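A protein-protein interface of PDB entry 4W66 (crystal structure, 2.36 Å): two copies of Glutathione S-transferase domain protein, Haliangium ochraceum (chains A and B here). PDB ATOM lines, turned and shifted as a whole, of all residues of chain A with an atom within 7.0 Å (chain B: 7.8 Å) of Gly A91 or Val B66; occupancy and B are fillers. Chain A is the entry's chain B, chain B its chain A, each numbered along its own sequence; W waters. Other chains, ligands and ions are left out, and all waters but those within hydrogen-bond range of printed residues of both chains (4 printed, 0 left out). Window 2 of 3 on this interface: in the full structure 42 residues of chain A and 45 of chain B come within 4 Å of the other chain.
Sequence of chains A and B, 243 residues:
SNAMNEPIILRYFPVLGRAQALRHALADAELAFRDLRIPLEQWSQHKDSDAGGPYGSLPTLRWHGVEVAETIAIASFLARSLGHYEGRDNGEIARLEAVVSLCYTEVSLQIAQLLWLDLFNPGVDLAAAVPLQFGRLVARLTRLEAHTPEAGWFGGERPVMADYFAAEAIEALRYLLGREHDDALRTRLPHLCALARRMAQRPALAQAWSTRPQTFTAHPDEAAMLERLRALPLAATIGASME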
ATOM      1  N   ARG A  88     -35.986 -23.200  34.464  1.00  0.00           N
ATOM      2  CA  ARG A  88     -35.177 -23.756  33.388  1.00  0.00           C
ATOM      3  C   ARG A  88     -34.425 -22.629  32.684  1.00  0.00           C
ATOM      4  O   ARG A  88     -34.996 -21.583  32.398  1.00  0.00           O
ATOM      5  CB  ARG A  88     -36.050 -24.518  32.379  1.00  0.00           C
ATOM      6  CG  ARG A  88     -37.197 -25.276  33.014  1.00  0.00           C
ATOM      7  CD  ARG A  88     -37.933 -26.154  32.014  1.00  0.00           C
ATOM      8  NE  ARG A  88     -37.528 -27.549  32.135  1.00  0.00           N
ATOM      9  CZ  ARG A  88     -38.279 -28.542  32.604  1.00  0.00           C
ATOM     10  NH1 ARG A  88     -39.539 -28.355  32.986  1.00  0.00           N
ATOM     11  NH2 ARG A  88     -37.750 -29.755  32.667  1.00  0.00           N
ATOM     12  N   ASP A  89     -33.145 -22.840  32.396  1.00  0.00           N
ATOM     13  CA  ASP A  89     -32.384 -21.849  31.644  1.00  0.00           C
ATOM     14  C   ASP A  89     -32.749 -21.878  30.152  1.00  0.00           C
ATOM     15  O   ASP A  89     -33.489 -22.756  29.690  1.00  0.00           O
ATOM     16  CB  ASP A  89     -30.879 -21.985  31.911  1.00  0.00           C
ATOM     17  CG  ASP A  89     -30.241 -23.219  31.280  1.00  0.00           C
ATOM     18  OD1 ASP A  89     -30.583 -23.616  30.151  1.00  0.00           O
ATOM     19  OD2 ASP A  89     -29.316 -23.771  31.906  1.00  0.00           O
ATOM     20  N   ASN A  90     -32.247 -20.906  29.402  1.00  0.00           N
ATOM     21  CA  ASN A  90     -32.676 -20.730  28.007  1.00  0.00           C
ATOM     22  C   ASN A  90     -32.288 -21.878  27.084  1.00  0.00           C
ATOM     23  O   ASN A  90     -33.008 -22.176  26.147  1.00  0.00           O
ATOM     24  CB  ASN A  90     -32.130 -19.420  27.442  1.00  0.00           C
ATOM     25  CG  ASN A  90     -32.736 -18.200  28.094  1.00  0.00           C
ATOM     26  OD1 ASN A  90     -33.842 -18.234  28.672  1.00  0.00           O
ATOM     27  ND2 ASN A  90     -32.019 -17.101  27.999  1.00  0.00           N
ATOM     28  N   GLY A  91     -31.139 -22.494  27.344  1.00  0.00           N
ATOM     29  CA  GLY A  91     -30.692 -23.687  26.625  1.00  0.00           C
ATOM     30  C   GLY A  91     -31.604 -24.882  26.856  1.00  0.00           C
ATOM     31  O   GLY A  91     -31.887 -25.627  25.908  1.00  0.00           O
ATOM     32  N   GLU A  92     -32.056 -25.045  28.111  1.00  0.00           N
ATOM     33  CA  GLU A  92     -33.021 -26.089  28.519  1.00  0.00           C
ATOM     34  C   GLU A  92     -34.368 -25.844  27.838  1.00  0.00           C
ATOM     35  O   GLU A  92     -34.967 -26.766  27.291  1.00  0.00           O
ATOM     36  CB  GLU A  92     -33.235 -26.116  30.050  1.00  0.00           C
ATOM     37  CG  GLU A  92     -32.212 -26.928  30.849  1.00  0.00           C
ATOM     38  CD  GLU A  92     -32.002 -26.466  32.313  1.00  0.00           C
ATOM     39  OE1 GLU A  92     -32.919 -25.868  32.923  1.00  0.00           O
ATOM     40  OE2 GLU A  92     -30.902 -26.712  32.874  1.00  0.00           O
ATOM     41  N   ILE A  93     -34.848 -24.605  27.879  1.00  0.00           N
ATOM     42  CA  ILE A  93     -36.111 -24.274  27.235  1.00  0.00           C
ATOM     43  C   ILE A  93     -36.037 -24.615  25.737  1.00  0.00           C
ATOM     44  O   ILE A  93     -36.996 -25.133  25.155  1.00  0.00           O
ATOM     45  CB  ILE A  93     -36.495 -22.796  27.444  1.00  0.00           C
ATOM     46  CG1 ILE A  93     -36.883 -22.560  28.904  1.00  0.00           C
ATOM     47  CG2 ILE A  93     -37.668 -22.403  26.557  1.00  0.00           C
ATOM     48  CD1 ILE A  93     -36.961 -21.096  29.308  1.00  0.00           C
ATOM     49  N   ALA A  94     -34.880 -24.376  25.134  1.00  0.00           N
ATOM     50  CA  ALA A  94     -34.728 -24.586  23.706  1.00  0.00           C
ATOM     51  C   ALA A  94     -34.628 -26.052  23.315  1.00  0.00           C
ATOM     52  O   ALA A  94     -34.954 -26.417  22.187  1.00  0.00           O
ATOM     53  CB  ALA A  94     -33.534 -23.806  23.173  1.00  0.00           C
ATOM     54  N   ARG A  95     -34.161 -26.889  24.221  1.00  0.00           N
ATOM     55  CA  ARG A  95     -34.210 -28.323  23.987  1.00  0.00           C
ATOM     56  C   ARG A  95     -35.628 -28.790  23.943  1.00  0.00           C
ATOM     57  O   ARG A  95     -35.984 -29.572  23.082  1.00  0.00           O
ATOM     58  CB  ARG A  95     -33.470 -29.107  25.070  1.00  0.00           C
ATOM     59  CG  ARG A  95     -31.966 -29.078  24.878  1.00  0.00           C
ATOM     60  CD  ARG A  95     -31.249 -30.101  25.748  1.00  0.00           C
ATOM     61  NE  ARG A  95     -30.157 -29.435  26.443  1.00  0.00           N
ATOM     62  CZ  ARG A  95     -30.164 -29.062  27.723  1.00  0.00           C
ATOM     63  NH1 ARG A  95     -31.198 -29.326  28.519  1.00  0.00           N
ATOM     64  NH2 ARG A  95     -29.103 -28.435  28.216  1.00  0.00           N
ATOM     65  N   LEU A  96     -36.434 -28.328  24.883  1.00  0.00           N
ATOM     66  CA  LEU A  96     -37.844 -28.673  24.887  1.00  0.00           C
ATOM     67  C   LEU A  96     -38.581 -28.160  23.659  1.00  0.00           C
ATOM     68  O   LEU A  96     -39.371 -28.882  23.066  1.00  0.00           O
ATOM     69  CB  LEU A  96     -38.520 -28.113  26.119  1.00  0.00           C
ATOM     70  CG  LEU A  96     -38.122 -28.731  27.448  1.00  0.00           C
ATOM     71  CD1 LEU A  96     -39.006 -28.107  28.521  1.00  0.00           C
ATOM     72  CD2 LEU A  96     -38.258 -30.243  27.442  1.00  0.00           C
ATOM     73  N   PRO B   7     -17.076 -17.614  19.736  1.00  0.00           N
ATOM     74  CA  PRO B   7     -17.940 -18.226  20.742  1.00  0.00           C
ATOM     75  C   PRO B   7     -19.407 -18.421  20.297  1.00  0.00           C
ATOM     76  O   PRO B   7     -20.117 -19.207  20.924  1.00  0.00           O
ATOM     77  CB  PRO B   7     -17.848 -17.253  21.920  1.00  0.00           C
ATOM     78  CG  PRO B   7     -17.429 -15.955  21.329  1.00  0.00           C
ATOM     79  CD  PRO B   7     -16.579 -16.291  20.150  1.00  0.00           C
ATOM     80  N   ILE B   9     -21.491 -19.815  16.999  1.00  0.00           N
ATOM     81  CA  ILE B   9     -21.337 -20.527  15.716  1.00  0.00           C
ATOM     82  C   ILE B   9     -22.703 -20.941  15.186  1.00  0.00           C
ATOM     83  O   ILE B   9     -23.429 -21.631  15.872  1.00  0.00           O
ATOM     84  CB  ILE B   9     -20.493 -21.806  15.852  1.00  0.00           C
ATOM     85  CG1 ILE B   9     -19.112 -21.515  16.436  1.00  0.00           C
ATOM     86  CG2 ILE B   9     -20.288 -22.487  14.498  1.00  0.00           C
ATOM     87  CD1 ILE B   9     -18.343 -22.770  16.787  1.00  0.00           C
ATOM     88  N   ARG B  11     -24.472 -23.086  12.205  1.00  0.00           N
ATOM     89  CA  ARG B  11     -24.100 -24.128  11.265  1.00  0.00           C
ATOM     90  C   ARG B  11     -25.259 -24.407  10.350  1.00  0.00           C
ATOM     91  O   ARG B  11     -26.373 -24.667  10.811  1.00  0.00           O
ATOM     92  CB  ARG B  11     -23.742 -25.419  11.992  1.00  0.00           C
ATOM     93  CG  ARG B  11     -22.755 -25.246  13.134  1.00  0.00           C
ATOM     94  CD  ARG B  11     -22.236 -26.594  13.584  1.00  0.00           C
ATOM     95  NE  ARG B  11     -21.506 -26.534  14.842  1.00  0.00           N
ATOM     96  CZ  ARG B  11     -22.054 -26.468  16.052  1.00  0.00           C
ATOM     97  NH1 ARG B  11     -23.375 -26.409  16.213  1.00  0.00           N
ATOM     98  NH2 ARG B  11     -21.266 -26.468  17.121  1.00  0.00           N
ATOM     99  N   THR B  60     -27.825 -25.712  13.307  1.00  0.00           N
ATOM    100  CA  THR B  60     -27.513 -25.693  14.731  1.00  0.00           C
ATOM    101  C   THR B  60     -26.789 -24.417  15.107  1.00  0.00           C
ATOM    102  O   THR B  60     -26.139 -23.784  14.284  1.00  0.00           O
ATOM    103  CB  THR B  60     -26.647 -26.882  15.204  1.00  0.00           C
ATOM    104  OG1 THR B  60     -25.471 -26.960  14.405  1.00  0.00           O
ATOM    105  CG2 THR B  60     -27.421 -28.199  15.122  1.00  0.00           C
ATOM    106  N   LEU B  61     -26.913 -24.064  16.378  1.00  0.00           N
ATOM    107  CA  LEU B  61     -26.245 -22.915  16.936  1.00  0.00           C
ATOM    108  C   LEU B  61     -25.464 -23.305  18.187  1.00  0.00           C
ATOM    109  O   LEU B  61     -25.953 -24.008  19.042  1.00  0.00           O
ATOM    110  CB  LEU B  61     -27.297 -21.874  17.307  1.00  0.00           C
ATOM    111  CG  LEU B  61     -26.868 -20.603  18.042  1.00  0.00           C
ATOM    112  CD1 LEU B  61     -26.208 -19.662  17.063  1.00  0.00           C
ATOM    113  CD2 LEU B  61     -28.063 -19.924  18.686  1.00  0.00           C
ATOM    114  N   ARG B  62     -24.242 -22.830  18.285  1.00  0.00           N
ATOM    115  CA  ARG B  62     -23.543 -22.828  19.531  1.00  0.00           C
ATOM    116  C   ARG B  62     -23.405 -21.382  19.991  1.00  0.00           C
ATOM    117  O   ARG B  62     -22.933 -20.516  19.251  1.00  0.00           O
ATOM    118  CB  ARG B  62     -22.199 -23.480  19.362  1.00  0.00           C
ATOM    119  CG  ARG B  62     -21.454 -23.676  20.661  1.00  0.00           C
ATOM    120  CD  ARG B  62     -20.027 -24.093  20.364  1.00  0.00           C
ATOM    121  NE  ARG B  62     -19.268 -24.295  21.584  1.00  0.00           N
ATOM    122  CZ  ARG B  62     -19.399 -25.352  22.382  1.00  0.00           C
ATOM    123  NH1 ARG B  62     -20.289 -26.297  22.103  1.00  0.00           N
ATOM    124  NH2 ARG B  62     -18.640 -25.466  23.471  1.00  0.00           N
ATOM    125  N   TRP B  63     -23.840 -21.152  21.223  1.00  0.00           N
ATOM    126  CA  TRP B  63     -23.898 -19.847  21.843  1.00  0.00           C
ATOM    127  C   TRP B  63     -23.191 -19.926  23.201  1.00  0.00           C
ATOM    128  O   TRP B  63     -23.759 -20.410  24.162  1.00  0.00           O
ATOM    129  CB  TRP B  63     -25.365 -19.448  22.021  1.00  0.00           C
ATOM    130  CG  TRP B  63     -25.591 -18.153  22.731  1.00  0.00           C
ATOM    131  CD1 TRP B  63     -25.640 -17.954  24.081  1.00  0.00           C
ATOM    132  CD2 TRP B  63     -25.815 -16.877  22.133  1.00  0.00           C
ATOM    133  NE1 TRP B  63     -25.882 -16.643  24.360  1.00  0.00           N
ATOM    134  CE2 TRP B  63     -25.995 -15.952  23.184  1.00  0.00           C
ATOM    135  CE3 TRP B  63     -25.893 -16.423  20.810  1.00  0.00           C
ATOM    136  CZ2 TRP B  63     -26.247 -14.594  22.958  1.00  0.00           C
ATOM    137  CZ3 TRP B  63     -26.149 -15.070  20.584  1.00  0.00           C
ATOM    138  CH2 TRP B  63     -26.319 -14.172  21.661  1.00  0.00           C
ATOM    139  N   HIS B  64     -21.934 -19.497  23.240  1.00  0.00           N
ATOM    140  CA  HIS B  64     -21.157 -19.426  24.469  1.00  0.00           C
ATOM    141  C   HIS B  64     -21.237 -20.712  25.267  1.00  0.00           C
ATOM    142  O   HIS B  64     -21.523 -20.679  26.458  1.00  0.00           O
ATOM    143  CB  HIS B  64     -21.651 -18.250  25.309  1.00  0.00           C
ATOM    144  CG  HIS B  64     -21.468 -16.935  24.635  1.00  0.00           C
ATOM    145  ND1 HIS B  64     -20.224 -16.393  24.414  1.00  0.00           N
ATOM    146  CD2 HIS B  64     -22.359 -16.074  24.098  1.00  0.00           C
ATOM    147  CE1 HIS B  64     -20.361 -15.247  23.769  1.00  0.00           C
ATOM    148  NE2 HIS B  64     -21.647 -15.037  23.555  1.00  0.00           N
ATOM    149  N   GLY B  65     -21.035 -21.844  24.593  1.00  0.00           N
ATOM    150  CA  GLY B  65     -21.052 -23.158  25.247  1.00  0.00           C
ATOM    151  C   GLY B  65     -22.371 -23.911  25.190  1.00  0.00           C
ATOM    152  O   GLY B  65     -22.396 -25.108  25.442  1.00  0.00           O
ATOM    153  N   VAL B  66     -23.466 -23.238  24.838  1.00  0.00           N
ATOM    154  CA  VAL B  66     -24.781 -23.860  24.823  1.00  0.00           C
ATOM    155  C   VAL B  66     -25.172 -24.247  23.401  1.00  0.00           C
ATOM    156  O   VAL B  66     -25.276 -23.389  22.536  1.00  0.00           O
ATOM    157  CB  VAL B  66     -25.846 -22.903  25.416  1.00  0.00           C
ATOM    158  CG1 VAL B  66     -27.266 -23.419  25.172  1.00  0.00           C
ATOM    159  CG2 VAL B  66     -25.604 -22.709  26.910  1.00  0.00           C
ATOM    160  N   GLU B  67     -25.403 -25.539  23.167  1.00  0.00           N
ATOM    161  CA  GLU B  67     -25.812 -26.036  21.838  1.00  0.00           C
ATOM    162  C   GLU B  67     -27.339 -25.991  21.694  1.00  0.00           C
ATOM    163  O   GLU B  67     -28.063 -26.326  22.620  1.00  0.00           O
ATOM    164  CB  GLU B  67     -25.282 -27.461  21.604  1.00  0.00           C
ATOM    165  CG  GLU B  67     -23.758 -27.554  21.453  1.00  0.00           C
ATOM    166  CD  GLU B  67     -23.219 -27.008  20.115  1.00  0.00           C
ATOM    167  OE1 GLU B  67     -24.006 -26.717  19.182  1.00  0.00           O
ATOM    168  OE2 GLU B  67     -21.975 -26.881  19.975  1.00  0.00           O
ATOM    169  N   VAL B  68     -27.810 -25.550  20.533  1.00  0.00           N
ATOM    170  CA  VAL B  68     -29.236 -25.397  20.250  1.00  0.00           C
ATOM    171  C   VAL B  68     -29.510 -25.962  18.857  1.00  0.00           C
ATOM    172  O   VAL B  68     -28.691 -25.788  17.976  1.00  0.00           O
ATOM    173  CB  VAL B  68     -29.639 -23.911  20.285  1.00  0.00           C
ATOM    174  CG1 VAL B  68     -31.147 -23.748  20.331  1.00  0.00           C
ATOM    175  CG2 VAL B  68     -29.018 -23.212  21.480  1.00  0.00           C
ATOM    176  N   ALA B  69     -30.649 -26.629  18.661  1.00  0.00           N
ATOM    177  CA  ALA B  69     -31.027 -27.194  17.341  1.00  0.00           C
ATOM    178  C   ALA B  69     -32.420 -26.770  16.880  1.00  0.00           C
ATOM    179  O   ALA B  69     -33.207 -26.280  17.670  1.00  0.00           O
ATOM    180  CB  ALA B  69     -30.945 -28.708  17.367  1.00  0.00           C
ATOM    181  N   PHE B  77     -34.694 -18.966  21.049  1.00  0.00           N
ATOM    182  CA  PHE B  77     -33.546 -18.874  21.931  1.00  0.00           C
ATOM    183  C   PHE B  77     -32.858 -17.525  21.716  1.00  0.00           C
ATOM    184  O   PHE B  77     -32.534 -16.829  22.673  1.00  0.00           O
ATOM    185  CB  PHE B  77     -32.586 -20.017  21.652  1.00  0.00           C
ATOM    186  CG  PHE B  77     -31.293 -19.916  22.388  1.00  0.00           C
ATOM    187  CD1 PHE B  77     -30.225 -19.222  21.847  1.00  0.00           C
ATOM    188  CD2 PHE B  77     -31.140 -20.511  23.623  1.00  0.00           C
ATOM    189  CE1 PHE B  77     -29.032 -19.113  22.528  1.00  0.00           C
ATOM    190  CE2 PHE B  77     -29.941 -20.422  24.306  1.00  0.00           C
ATOM    191  CZ  PHE B  77     -28.884 -19.729  23.751  1.00  0.00           C
ATOM    192  N   ARG B  80     -34.909 -14.560  23.101  1.00  0.00           N
ATOM    193  CA  ARG B  80     -34.621 -14.448  24.533  1.00  0.00           C
ATOM    194  C   ARG B  80     -33.249 -13.884  24.796  1.00  0.00           C
ATOM    195  O   ARG B  80     -33.097 -13.010  25.620  1.00  0.00           O
ATOM    196  CB  ARG B  80     -34.708 -15.799  25.241  1.00  0.00           C
ATOM    197  CG  ARG B  80     -36.117 -16.333  25.363  1.00  0.00           C
ATOM    198  CD  ARG B  80     -36.181 -17.665  26.090  1.00  0.00           C
ATOM    199  NE  ARG B  80     -37.572 -18.097  26.097  1.00  0.00           N
ATOM    200  CZ  ARG B  80     -38.131 -18.937  25.231  1.00  0.00           C
ATOM    201  NH1 ARG B  80     -37.424 -19.533  24.287  1.00  0.00           N
ATOM    202  NH2 ARG B  80     -39.427 -19.205  25.339  1.00  0.00           N
ATOM    203  N   SER B  81     -32.251 -14.405  24.107  1.00  0.00           N
ATOM    204  CA  SER B  81     -30.869 -13.993  24.326  1.00  0.00           C
ATOM    205  C   SER B  81     -30.581 -12.534  23.942  1.00  0.00           C
ATOM    206  O   SER B  81     -29.767 -11.899  24.575  1.00  0.00           O
ATOM    207  CB  SER B  81     -29.928 -14.925  23.553  1.00  0.00           C
ATOM    208  OG  SER B  81     -30.064 -16.273  24.014  1.00  0.00           O
HETATM  209  O   HOH W   1     -29.404 -17.189  26.394  1.00  0.00           O
HETATM  210  O   HOH W   2     -32.274 -26.823  21.251  1.00  0.00           O
HETATM  211  O   HOH W   3     -35.021 -20.687  24.590  1.00  0.00           O
HETATM  212  O   HOH W   4     -30.698 -26.183  23.357  1.00  0.00           O
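The backbone carbonyl oxygen (O) of Leu B61 lies within hydrogen-bond range of the backbone NH (N) of Val B68 (2.8 Å).
The side-chain carboxylate of Asp A89 lies within hydrogen-bond range of the backbone NH of Gly A91 (3.1 Å).
The backbone carbonyl oxygen (O) of Phe B77 lies within hydrogen-bond range of the side-chain hydroxyl (OG) of Ser B81 (2.9 Å).
Among the printed residues, merely in contact across the chains: Asn A90 with Arg B80 (3.5 Å), Asn A90 with Phe B77 (3.6 Å), Ile A93 with Arg B80 (3.7 Å), Ala A94 with Val B68 (3.7 Å), Gly A91 with Val B66 (3.7 Å) and Gly A91 with Phe B77 (3.9 Å).
Printed residues of chain B within 4 Å of Asn A90: Phe B77 (3.6 Å) and Arg B80 (3.5 Å).
Gly A91 touches just these residues of chain B: Val B66 (3.7 Å) and Phe B77 (3.9 Å).
Of the printed residues of chain B, Ala A94 touches Val B68.
Gly B65 touches none of the printed residues of chain A.
Of chain A, only Gly A91 (3.7 Å) comes within 4 Å of Val B66.
The nearest residue of chain B that does not touch Gly A91 is Glu B67 (5.1 Å).
Of the 16 printed residues of chain B, 4 touch a printed residue of chain A.
Of the 9 printed residues of chain A, 4 touch a printed residue of chain B.
Hydrophobic or aromatic side chains of chain A within 4 Å of the printed part of chain B: Ile A93 and Ala A94.
Along chain A the printed residues that touch a printed residue of chain B span positions 90 to 94.
No position is printed for both chains.
Of the 6 pairs that touch across the chains among the printed residues, none has its exchanged pair printed and touching as well.
Water W1 lies within hydrogen-bond range of the side-chain hydroxyl (OG) of Ser B81 and the side-chain amide nitrogen (ND2) of Asn A90.
Water W3 bridges the guanidinium group of Arg B80 (2.7 Å) and the backbone carbonyl oxygen of Asn A90 (2.9 Å).
Water W4 lies within hydrogen-bond range of O of Glu B67 (2.7 Å) and O of Gly A91 (2.9 Å).
Water W2 lies within hydrogen-bond range of O of Ala A94 (2.9 Å) and N of Ala B69 (3.1 Å).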
